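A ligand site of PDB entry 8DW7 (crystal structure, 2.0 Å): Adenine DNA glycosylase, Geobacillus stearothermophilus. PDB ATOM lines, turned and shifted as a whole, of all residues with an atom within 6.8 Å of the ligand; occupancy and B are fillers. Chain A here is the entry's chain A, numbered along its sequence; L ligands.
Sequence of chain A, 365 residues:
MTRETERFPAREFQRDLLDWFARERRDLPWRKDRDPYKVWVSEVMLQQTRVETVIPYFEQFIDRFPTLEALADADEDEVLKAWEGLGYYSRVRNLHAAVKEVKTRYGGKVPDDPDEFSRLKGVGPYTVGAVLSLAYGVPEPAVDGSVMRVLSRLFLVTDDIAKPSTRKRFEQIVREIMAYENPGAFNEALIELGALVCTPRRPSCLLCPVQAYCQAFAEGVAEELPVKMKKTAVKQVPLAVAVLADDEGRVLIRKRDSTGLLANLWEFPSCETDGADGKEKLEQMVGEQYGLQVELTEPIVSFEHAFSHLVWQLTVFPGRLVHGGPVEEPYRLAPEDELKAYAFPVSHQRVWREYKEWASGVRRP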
ATOM      1  N   PHE A  13     -21.622  16.992  11.790  1.00  0.00           N
ATOM      2  CA  PHE A  13     -21.131  16.916  13.169  1.00  0.00           C
ATOM      3  C   PHE A  13     -19.604  16.818  13.168  1.00  0.00           C
ATOM      4  O   PHE A  13     -18.937  17.645  13.786  1.00  0.00           O
ATOM      5  CB  PHE A  13     -21.769  15.733  13.909  1.00  0.00           C
ATOM      6  CG  PHE A  13     -21.310  15.578  15.308  1.00  0.00           C
ATOM      7  CD1 PHE A  13     -21.886  16.344  16.347  1.00  0.00           C
ATOM      8  CD2 PHE A  13     -20.331  14.695  15.624  1.00  0.00           C
ATOM      9  CE1 PHE A  13     -21.466  16.192  17.715  1.00  0.00           C
ATOM     10  CE2 PHE A  13     -19.861  14.541  17.005  1.00  0.00           C
ATOM     11  CZ  PHE A  13     -20.447  15.329  18.040  1.00  0.00           C
ATOM     12  N   ARG A 149     -20.658  11.956  29.178  1.00  0.00           N
ATOM     13  CA  ARG A 149     -21.552  13.111  29.482  1.00  0.00           C
ATOM     14  C   ARG A 149     -21.965  13.811  28.191  1.00  0.00           C
ATOM     15  O   ARG A 149     -23.156  14.114  27.958  1.00  0.00           O
ATOM     16  CB  ARG A 149     -20.846  14.087  30.426  1.00  0.00           C
ATOM     17  CG  ARG A 149     -21.405  15.491  30.434  1.00  0.00           C
ATOM     18  CD  ARG A 149     -20.791  16.332  31.606  1.00  0.00           C
ATOM     19  NE  ARG A 149     -19.393  16.644  31.364  1.00  0.00           N
ATOM     20  CZ  ARG A 149     -18.388  16.036  31.938  1.00  0.00           C
ATOM     21  NH1 ARG A 149     -18.574  15.052  32.783  1.00  0.00           N
ATOM     22  NH2 ARG A 149     -17.166  16.386  31.598  1.00  0.00           N
ATOM     23  N   VAL A 150     -20.985  14.067  27.333  1.00  0.00           N
ATOM     24  CA  VAL A 150     -21.239  14.684  26.031  1.00  0.00           C
ATOM     25  C   VAL A 150     -22.247  13.845  25.244  1.00  0.00           C
ATOM     26  O   VAL A 150     -23.224  14.373  24.684  1.00  0.00           O
ATOM     27  CB  VAL A 150     -19.925  14.829  25.281  1.00  0.00           C
ATOM     28  CG1 VAL A 150     -20.181  15.263  23.812  1.00  0.00           C
ATOM     29  CG2 VAL A 150     -19.015  15.806  25.989  1.00  0.00           C
ATOM     30  N   ARG A 153     -25.846  13.881  26.489  1.00  0.00           N
ATOM     31  CA  ARG A 153     -26.518  15.126  26.139  1.00  0.00           C
ATOM     32  C   ARG A 153     -26.848  15.165  24.662  1.00  0.00           C
ATOM     33  O   ARG A 153     -28.022  15.396  24.283  1.00  0.00           O
ATOM     34  CB  ARG A 153     -25.638  16.318  26.566  1.00  0.00           C
ATOM     35  CG  ARG A 153     -25.666  16.503  28.132  1.00  0.00           C
ATOM     36  CD  ARG A 153     -24.615  17.465  28.615  1.00  0.00           C
ATOM     37  NE  ARG A 153     -24.679  17.591  30.068  1.00  0.00           N
ATOM     38  CZ  ARG A 153     -23.824  18.308  30.767  1.00  0.00           C
ATOM     39  NH1 ARG A 153     -22.803  18.919  30.177  1.00  0.00           N
ATOM     40  NH2 ARG A 153     -23.991  18.440  32.074  1.00  0.00           N
ATOM     41  N   LEU A 154     -25.856  14.918  23.811  1.00  0.00           N
ATOM     42  CA  LEU A 154     -26.110  14.955  22.362  1.00  0.00           C
ATOM     43  C   LEU A 154     -27.265  14.062  21.976  1.00  0.00           C
ATOM     44  O   LEU A 154     -28.128  14.453  21.185  1.00  0.00           O
ATOM     45  CB  LEU A 154     -24.871  14.572  21.593  1.00  0.00           C
ATOM     46  CG  LEU A 154     -23.792  15.644  21.580  1.00  0.00           C
ATOM     47  CD1 LEU A 154     -22.597  15.110  20.895  1.00  0.00           C
ATOM     48  CD2 LEU A 154     -24.233  16.906  20.888  1.00  0.00           C
ATOM     49  N   LEU A 193     -13.956  18.391  24.117  1.00  0.00           N
ATOM     50  CA  LEU A 193     -15.214  19.088  24.239  1.00  0.00           C
ATOM     51  C   LEU A 193     -15.750  18.969  25.663  1.00  0.00           C
ATOM     52  O   LEU A 193     -16.216  19.975  26.234  1.00  0.00           O
ATOM     53  CB  LEU A 193     -16.235  18.519  23.257  1.00  0.00           C
ATOM     54  CG  LEU A 193     -17.581  19.225  23.190  1.00  0.00           C
ATOM     55  CD1 LEU A 193     -17.383  20.548  22.466  1.00  0.00           C
ATOM     56  CD2 LEU A 193     -18.584  18.381  22.415  1.00  0.00           C
ATOM     57  N   VAL A 197     -15.888  22.785  27.329  1.00  0.00           N
ATOM     58  CA  VAL A 197     -17.134  23.335  26.875  1.00  0.00           C
ATOM     59  C   VAL A 197     -18.302  22.663  27.583  1.00  0.00           C
ATOM     60  O   VAL A 197     -19.009  23.300  28.355  1.00  0.00           O
ATOM     61  CB  VAL A 197     -17.271  23.201  25.333  1.00  0.00           C
ATOM     62  CG1 VAL A 197     -18.681  23.609  24.892  1.00  0.00           C
ATOM     63  CG2 VAL A 197     -16.163  24.055  24.599  1.00  0.00           C
ATOM     64  N   CYS A 198     -18.514  21.367  27.305  1.00  0.00           N
ATOM     65  CA  CYS A 198     -19.671  20.598  27.818  1.00  0.00           C
ATOM     66  C   CYS A 198     -19.343  20.005  29.190  1.00  0.00           C
ATOM     67  O   CYS A 198     -19.263  18.810  29.382  1.00  0.00           O
ATOM     68  CB  CYS A 198     -20.096  19.572  26.808  1.00  0.00           C
ATOM     69  SG  CYS A 198     -21.538  18.621  27.106  1.00  0.00           S
ATOM     70  N   THR A 199     -19.244  20.903  30.172  1.00  0.00           N
ATOM     71  CA  THR A 199     -18.782  20.639  31.512  1.00  0.00           C
ATOM     72  C   THR A 199     -19.945  20.106  32.384  1.00  0.00           C
ATOM     73  O   THR A 199     -21.125  20.259  32.040  1.00  0.00           O
ATOM     74  CB  THR A 199     -18.181  21.918  32.139  1.00  0.00           C
ATOM     75  OG1 THR A 199     -19.103  23.032  32.093  1.00  0.00           O
ATOM     76  CG2 THR A 199     -16.926  22.324  31.415  1.00  0.00           C
ATOM     77  N   PRO A 203     -22.704  23.980  31.459  1.00  0.00           N
ATOM     78  CA  PRO A 203     -22.065  23.839  30.153  1.00  0.00           C
ATOM     79  C   PRO A 203     -22.209  25.103  29.305  1.00  0.00           C
ATOM     80  O   PRO A 203     -23.246  25.783  29.324  1.00  0.00           O
ATOM     81  CB  PRO A 203     -22.795  22.660  29.523  1.00  0.00           C
ATOM     82  CG  PRO A 203     -24.079  22.576  30.239  1.00  0.00           C
ATOM     83  CD  PRO A 203     -23.795  22.988  31.628  1.00  0.00           C
ATOM     84  N   SER A 204     -21.144  25.412  28.557  1.00  0.00           N
ATOM     85  CA  SER A 204     -21.090  26.612  27.708  1.00  0.00           C
ATOM     86  C   SER A 204     -21.709  26.355  26.349  1.00  0.00           C
ATOM     87  O   SER A 204     -21.065  26.531  25.317  1.00  0.00           O
ATOM     88  CB  SER A 204     -19.641  27.061  27.548  1.00  0.00           C
ATOM     89  OG  SER A 204     -18.946  26.917  28.779  1.00  0.00           O
ATOM     90  N   CYS A 205     -22.977  25.952  26.373  1.00  0.00           N
ATOM     91  CA  CYS A 205     -23.672  25.562  25.134  1.00  0.00           C
ATOM     92  C   CYS A 205     -23.647  26.682  24.080  1.00  0.00           C
ATOM     93  O   CYS A 205     -23.567  26.414  22.871  1.00  0.00           O
ATOM     94  CB  CYS A 205     -25.112  25.149  25.457  1.00  0.00           C
ATOM     95  SG  CYS A 205     -25.388  24.014  26.908  1.00  0.00           S
ATOM     96  N   LEU A 206     -23.678  27.928  24.483  1.00  0.00           N
ATOM     97  CA  LEU A 206     -23.602  28.990  23.484  1.00  0.00           C
ATOM     98  C   LEU A 206     -22.211  29.080  22.845  1.00  0.00           C
ATOM     99  O   LEU A 206     -22.089  29.629  21.756  1.00  0.00           O
ATOM    100  CB  LEU A 206     -23.992  30.311  24.128  1.00  0.00           C
ATOM    101  CG  LEU A 206     -25.415  30.362  24.674  1.00  0.00           C
ATOM    102  CD1 LEU A 206     -25.622  31.657  25.441  1.00  0.00           C
ATOM    103  CD2 LEU A 206     -26.423  30.235  23.524  1.00  0.00           C
ATOM    104  N   LEU A 207     -21.177  28.591  23.503  1.00  0.00           N
ATOM    105  CA  LEU A 207     -19.845  28.521  22.934  1.00  0.00           C
ATOM    106  C   LEU A 207     -19.574  27.174  22.219  1.00  0.00           C
ATOM    107  O   LEU A 207     -18.411  26.900  21.897  1.00  0.00           O
ATOM    108  CB  LEU A 207     -18.786  28.691  24.034  1.00  0.00           C
ATOM    109  CG  LEU A 207     -18.324  30.097  24.393  1.00  0.00           C
ATOM    110  CD1 LEU A 207     -17.245  29.955  25.476  1.00  0.00           C
ATOM    111  CD2 LEU A 207     -17.782  30.833  23.185  1.00  0.00           C
ATOM    112  N   CYS A 208     -20.603  26.339  22.051  1.00  0.00           N
ATOM    113  CA  CYS A 208     -20.424  24.939  21.701  1.00  0.00           C
ATOM    114  C   CYS A 208     -20.501  24.771  20.196  1.00  0.00           C
ATOM    115  O   CYS A 208     -21.512  25.174  19.584  1.00  0.00           O
ATOM    116  CB  CYS A 208     -21.464  24.053  22.359  1.00  0.00           C
ATOM    117  SG  CYS A 208     -21.287  22.309  21.971  1.00  0.00           S
ATOM    118  N   PRO A 209     -19.483  24.225  19.579  1.00  0.00           N
ATOM    119  CA  PRO A 209     -19.531  24.016  18.127  1.00  0.00           C
ATOM    120  C   PRO A 209     -20.540  23.006  17.674  1.00  0.00           C
ATOM    121  O   PRO A 209     -20.799  22.934  16.481  1.00  0.00           O
ATOM    122  CB  PRO A 209     -18.130  23.525  17.786  1.00  0.00           C
ATOM    123  CG  PRO A 209     -17.759  22.729  19.055  1.00  0.00           C
ATOM    124  CD  PRO A 209     -18.289  23.614  20.188  1.00  0.00           C
ATOM    125  N   VAL A 210     -21.107  22.175  18.549  1.00  0.00           N
ATOM    126  CA  VAL A 210     -22.046  21.154  18.114  1.00  0.00           C
ATOM    127  C   VAL A 210     -23.428  21.386  18.701  1.00  0.00           C
ATOM    128  O   VAL A 210     -24.272  20.505  18.695  1.00  0.00           O
ATOM    129  CB  VAL A 210     -21.549  19.711  18.419  1.00  0.00           C
ATOM    130  CG1 VAL A 210     -20.308  19.445  17.557  1.00  0.00           C
ATOM    131  CG2 VAL A 210     -21.221  19.511  19.889  1.00  0.00           C
ATOM    132  N   GLN A 211     -23.669  22.623  19.169  1.00  0.00           N
ATOM    133  CA  GLN A 211     -24.958  22.996  19.744  1.00  0.00           C
ATOM    134  C   GLN A 211     -26.098  22.641  18.818  1.00  0.00           C
ATOM    135  O   GLN A 211     -27.192  22.269  19.280  1.00  0.00           O
ATOM    136  CB  GLN A 211     -24.913  24.485  20.063  1.00  0.00           C
ATOM    137  CG  GLN A 211     -26.186  25.058  20.599  1.00  0.00           C
ATOM    138  CD  GLN A 211     -26.311  26.516  20.230  1.00  0.00           C
ATOM    139  OE1 GLN A 211     -27.145  26.884  19.411  1.00  0.00           O
ATOM    140  NE2 GLN A 211     -25.466  27.333  20.819  1.00  0.00           N
ATOM    141  N   ALA A 212     -25.882  22.749  17.531  1.00  0.00           N
ATOM    142  CA  ALA A 212     -26.968  22.479  16.586  1.00  0.00           C
ATOM    143  C   ALA A 212     -27.356  21.006  16.543  1.00  0.00           C
ATOM    144  O   ALA A 212     -28.451  20.677  16.099  1.00  0.00           O
ATOM    145  CB  ALA A 212     -26.583  22.960  15.182  1.00  0.00           C
ATOM    146  N   TYR A 213     -26.526  20.123  17.017  1.00  0.00           N
ATOM    147  CA  TYR A 213     -26.824  18.701  16.977  1.00  0.00           C
ATOM    148  C   TYR A 213     -27.255  18.117  18.325  1.00  0.00           C
ATOM    149  O   TYR A 213     -27.457  16.900  18.427  1.00  0.00           O
ATOM    150  CB  TYR A 213     -25.600  17.955  16.496  1.00  0.00           C
ATOM    151  CG  TYR A 213     -24.912  18.618  15.318  1.00  0.00           C
ATOM    152  CD1 TYR A 213     -23.962  19.576  15.515  1.00  0.00           C
ATOM    153  CD2 TYR A 213     -25.218  18.254  14.003  1.00  0.00           C
ATOM    154  CE1 TYR A 213     -23.347  20.169  14.449  1.00  0.00           C
ATOM    155  CE2 TYR A 213     -24.596  18.824  12.965  1.00  0.00           C
ATOM    156  CZ  TYR A 213     -23.659  19.788  13.187  1.00  0.00           C
ATOM    157  OH  TYR A 213     -23.021  20.401  12.120  1.00  0.00           O
ATOM    158  N   CYS A 214     -27.394  18.957  19.362  1.00  0.00           N
ATOM    159  CA  CYS A 214     -27.526  18.512  20.744  1.00  0.00           C
ATOM    160  C   CYS A 214     -28.982  18.432  21.114  1.00  0.00           C
ATOM    161  O   CYS A 214     -29.685  19.467  21.134  1.00  0.00           O
ATOM    162  CB  CYS A 214     -26.779  19.461  21.677  1.00  0.00           C
ATOM    163  SG  CYS A 214     -26.665  18.892  23.321  1.00  0.00           S
ATOM    164  N   GLN A 215     -29.447  17.217  21.433  1.00  0.00           N
ATOM    165  CA  GLN A 215     -30.834  17.033  21.890  1.00  0.00           C
ATOM    166  C   GLN A 215     -31.089  17.580  23.288  1.00  0.00           C
ATOM    167  O   GLN A 215     -32.225  17.941  23.619  1.00  0.00           O
ATOM    168  CB  GLN A 215     -31.170  15.546  21.839  1.00  0.00           C
ATOM    169  CG  GLN A 215     -31.611  15.077  20.484  1.00  0.00           C
ATOM    170  CD  GLN A 215     -31.953  13.619  20.463  1.00  0.00           C
ATOM    171  OE1 GLN A 215     -32.844  13.152  21.198  1.00  0.00           O
ATOM    172  NE2 GLN A 215     -31.245  12.869  19.614  1.00  0.00           N
ATOM    173  N   ALA A 216     -30.086  17.561  24.174  1.00  0.00           N
ATOM    174  CA  ALA A 216     -30.322  18.022  25.524  1.00  0.00           C
ATOM    175  C   ALA A 216     -30.430  19.545  25.542  1.00  0.00           C
ATOM    176  O   ALA A 216     -31.256  20.120  26.245  1.00  0.00           O
ATOM    177  CB  ALA A 216     -29.226  17.543  26.476  1.00  0.00           C
ATOM    178  N   PHE A 217     -29.607  20.201  24.714  1.00  0.00           N
ATOM    179  CA  PHE A 217     -29.741  21.623  24.502  1.00  0.00           C
ATOM    180  C   PHE A 217     -31.155  21.974  24.032  1.00  0.00           C
ATOM    181  O   PHE A 217     -31.831  22.812  24.638  1.00  0.00           O
ATOM    182  CB  PHE A 217     -28.696  22.090  23.478  1.00  0.00           C
ATOM    183  CG  PHE A 217     -28.814  23.534  23.116  1.00  0.00           C
ATOM    184  CD1 PHE A 217     -28.559  24.526  24.062  1.00  0.00           C
ATOM    185  CD2 PHE A 217     -29.205  23.902  21.848  1.00  0.00           C
ATOM    186  CE1 PHE A 217     -28.696  25.850  23.740  1.00  0.00           C
ATOM    187  CE2 PHE A 217     -29.351  25.262  21.519  1.00  0.00           C
ATOM    188  CZ  PHE A 217     -29.083  26.223  22.464  1.00  0.00           C
ATOM    189  N   ALA A 222     -29.706  19.595  29.685  1.00  0.00           N
ATOM    190  CA  ALA A 222     -28.318  19.261  29.738  1.00  0.00           C
ATOM    191  C   ALA A 222     -27.842  18.984  31.156  1.00  0.00           C
ATOM    192  O   ALA A 222     -27.040  18.068  31.379  1.00  0.00           O
ATOM    193  CB  ALA A 222     -27.489  20.390  29.133  1.00  0.00           C
ATOM    194  N   GLU A 223     -28.289  19.766  32.131  1.00  0.00           N
ATOM    195  CA  GLU A 223     -27.730  19.661  33.474  1.00  0.00           C
ATOM    196  C   GLU A 223     -28.317  18.492  34.264  1.00  0.00           C
ATOM    197  O   GLU A 223     -27.787  18.144  35.330  1.00  0.00           O
ATOM    198  CB  GLU A 223     -27.932  20.961  34.233  1.00  0.00           C
ATOM    199  CG  GLU A 223     -27.573  22.177  33.456  1.00  0.00           C
ATOM    200  CD  GLU A 223     -26.872  23.222  34.284  1.00  0.00           C
ATOM    201  OE1 GLU A 223     -25.716  22.972  34.735  1.00  0.00           O
ATOM    202  OE2 GLU A 223     -27.468  24.302  34.515  1.00  0.00           O
HETATM  203 FE1  LIG L   1     -22.655  21.466  23.479  1.00  0.00          FE
HETATM  204 FE2  LIG L   1     -24.270  22.223  25.567  1.00  0.00          FE
HETATM  205 FE3  LIG L   1     -22.805  19.960  25.758  1.00  0.00          FE
HETATM  206 FE4  LIG L   1     -24.857  20.014  24.065  1.00  0.00          FE
HETATM  207  S1  LIG L   1     -24.943  20.193  26.316  1.00  0.00           S
HETATM  208  S2  LIG L   1     -22.835  19.201  23.563  1.00  0.00           S
HETATM  209  S3  LIG L   1     -24.758  22.229  23.341  1.00  0.00           S
HETATM  210  S4  LIG L   1     -21.976  22.115  25.595  1.00  0.00           S
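SG of Cys 208 binds FE1 of the ligand (2.2 Å).
An iron atom (FE4) of the ligand is bound by the side-chain sulfur (SG) of Cys 214, 2.3 Å away.
SG of Cys 198 binds FE3 of the ligand (2.3 Å).
FE2 of the ligand is bound by SG of Cys 205, at 2.5 Å.
N of Phe 217 sits close to SG of Cys 214 (3.5 Å).
The side-chain sulfur (SG) of Cys 198 lies close to the guanidinium group (NH1) of Arg 153.
The backbone carbonyl oxygen of Cys 205 is in hydrogen-bond range of the side-chain amide nitrogen of Gln 211, at 2.9 Å.
The side-chain sulfur (SG) of Cys 205 sits close to the backbone carbonyl oxygen (O) of Pro 203, at 3.7 Å.
O of Ala 222 lies within hydrogen-bond range of NE of Arg 153 (2.7 Å).
The guanidinium group (NH1) of Arg 153 sits at hydrogen-bond distance from the backbone carbonyl oxygen (O) of Thr 199 (2.8 Å).
The backbone carbonyl oxygen of Val 197 is in hydrogen-bond range of the backbone NH of Ser 204.
O of Leu 154 lies within hydrogen-bond range of N of Gln 215.
Arg 153 touches the ligand.
Leu 154 touches the ligand.
CG1 of Val 197 touches S4 of the ligand, 3.7 Å away.
Gln 211 touches the ligand (CA to S3, 3.7 Å).
CB of Phe 217 touches S3 of the ligand, 3.9 Å away.
Ala 222 touches the ligand.
Hydrophobic or aromatic side chains within 4 Å of the ligand: Leu 154, Val 197, Phe 217 and Ala 222.
Within 4 Å of the ligand: Arg 153, Leu 154, Val 197, Cys 198, Cys 205, Cys 208, Gln 211, Cys 214, Phe 217 and Ala 222.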
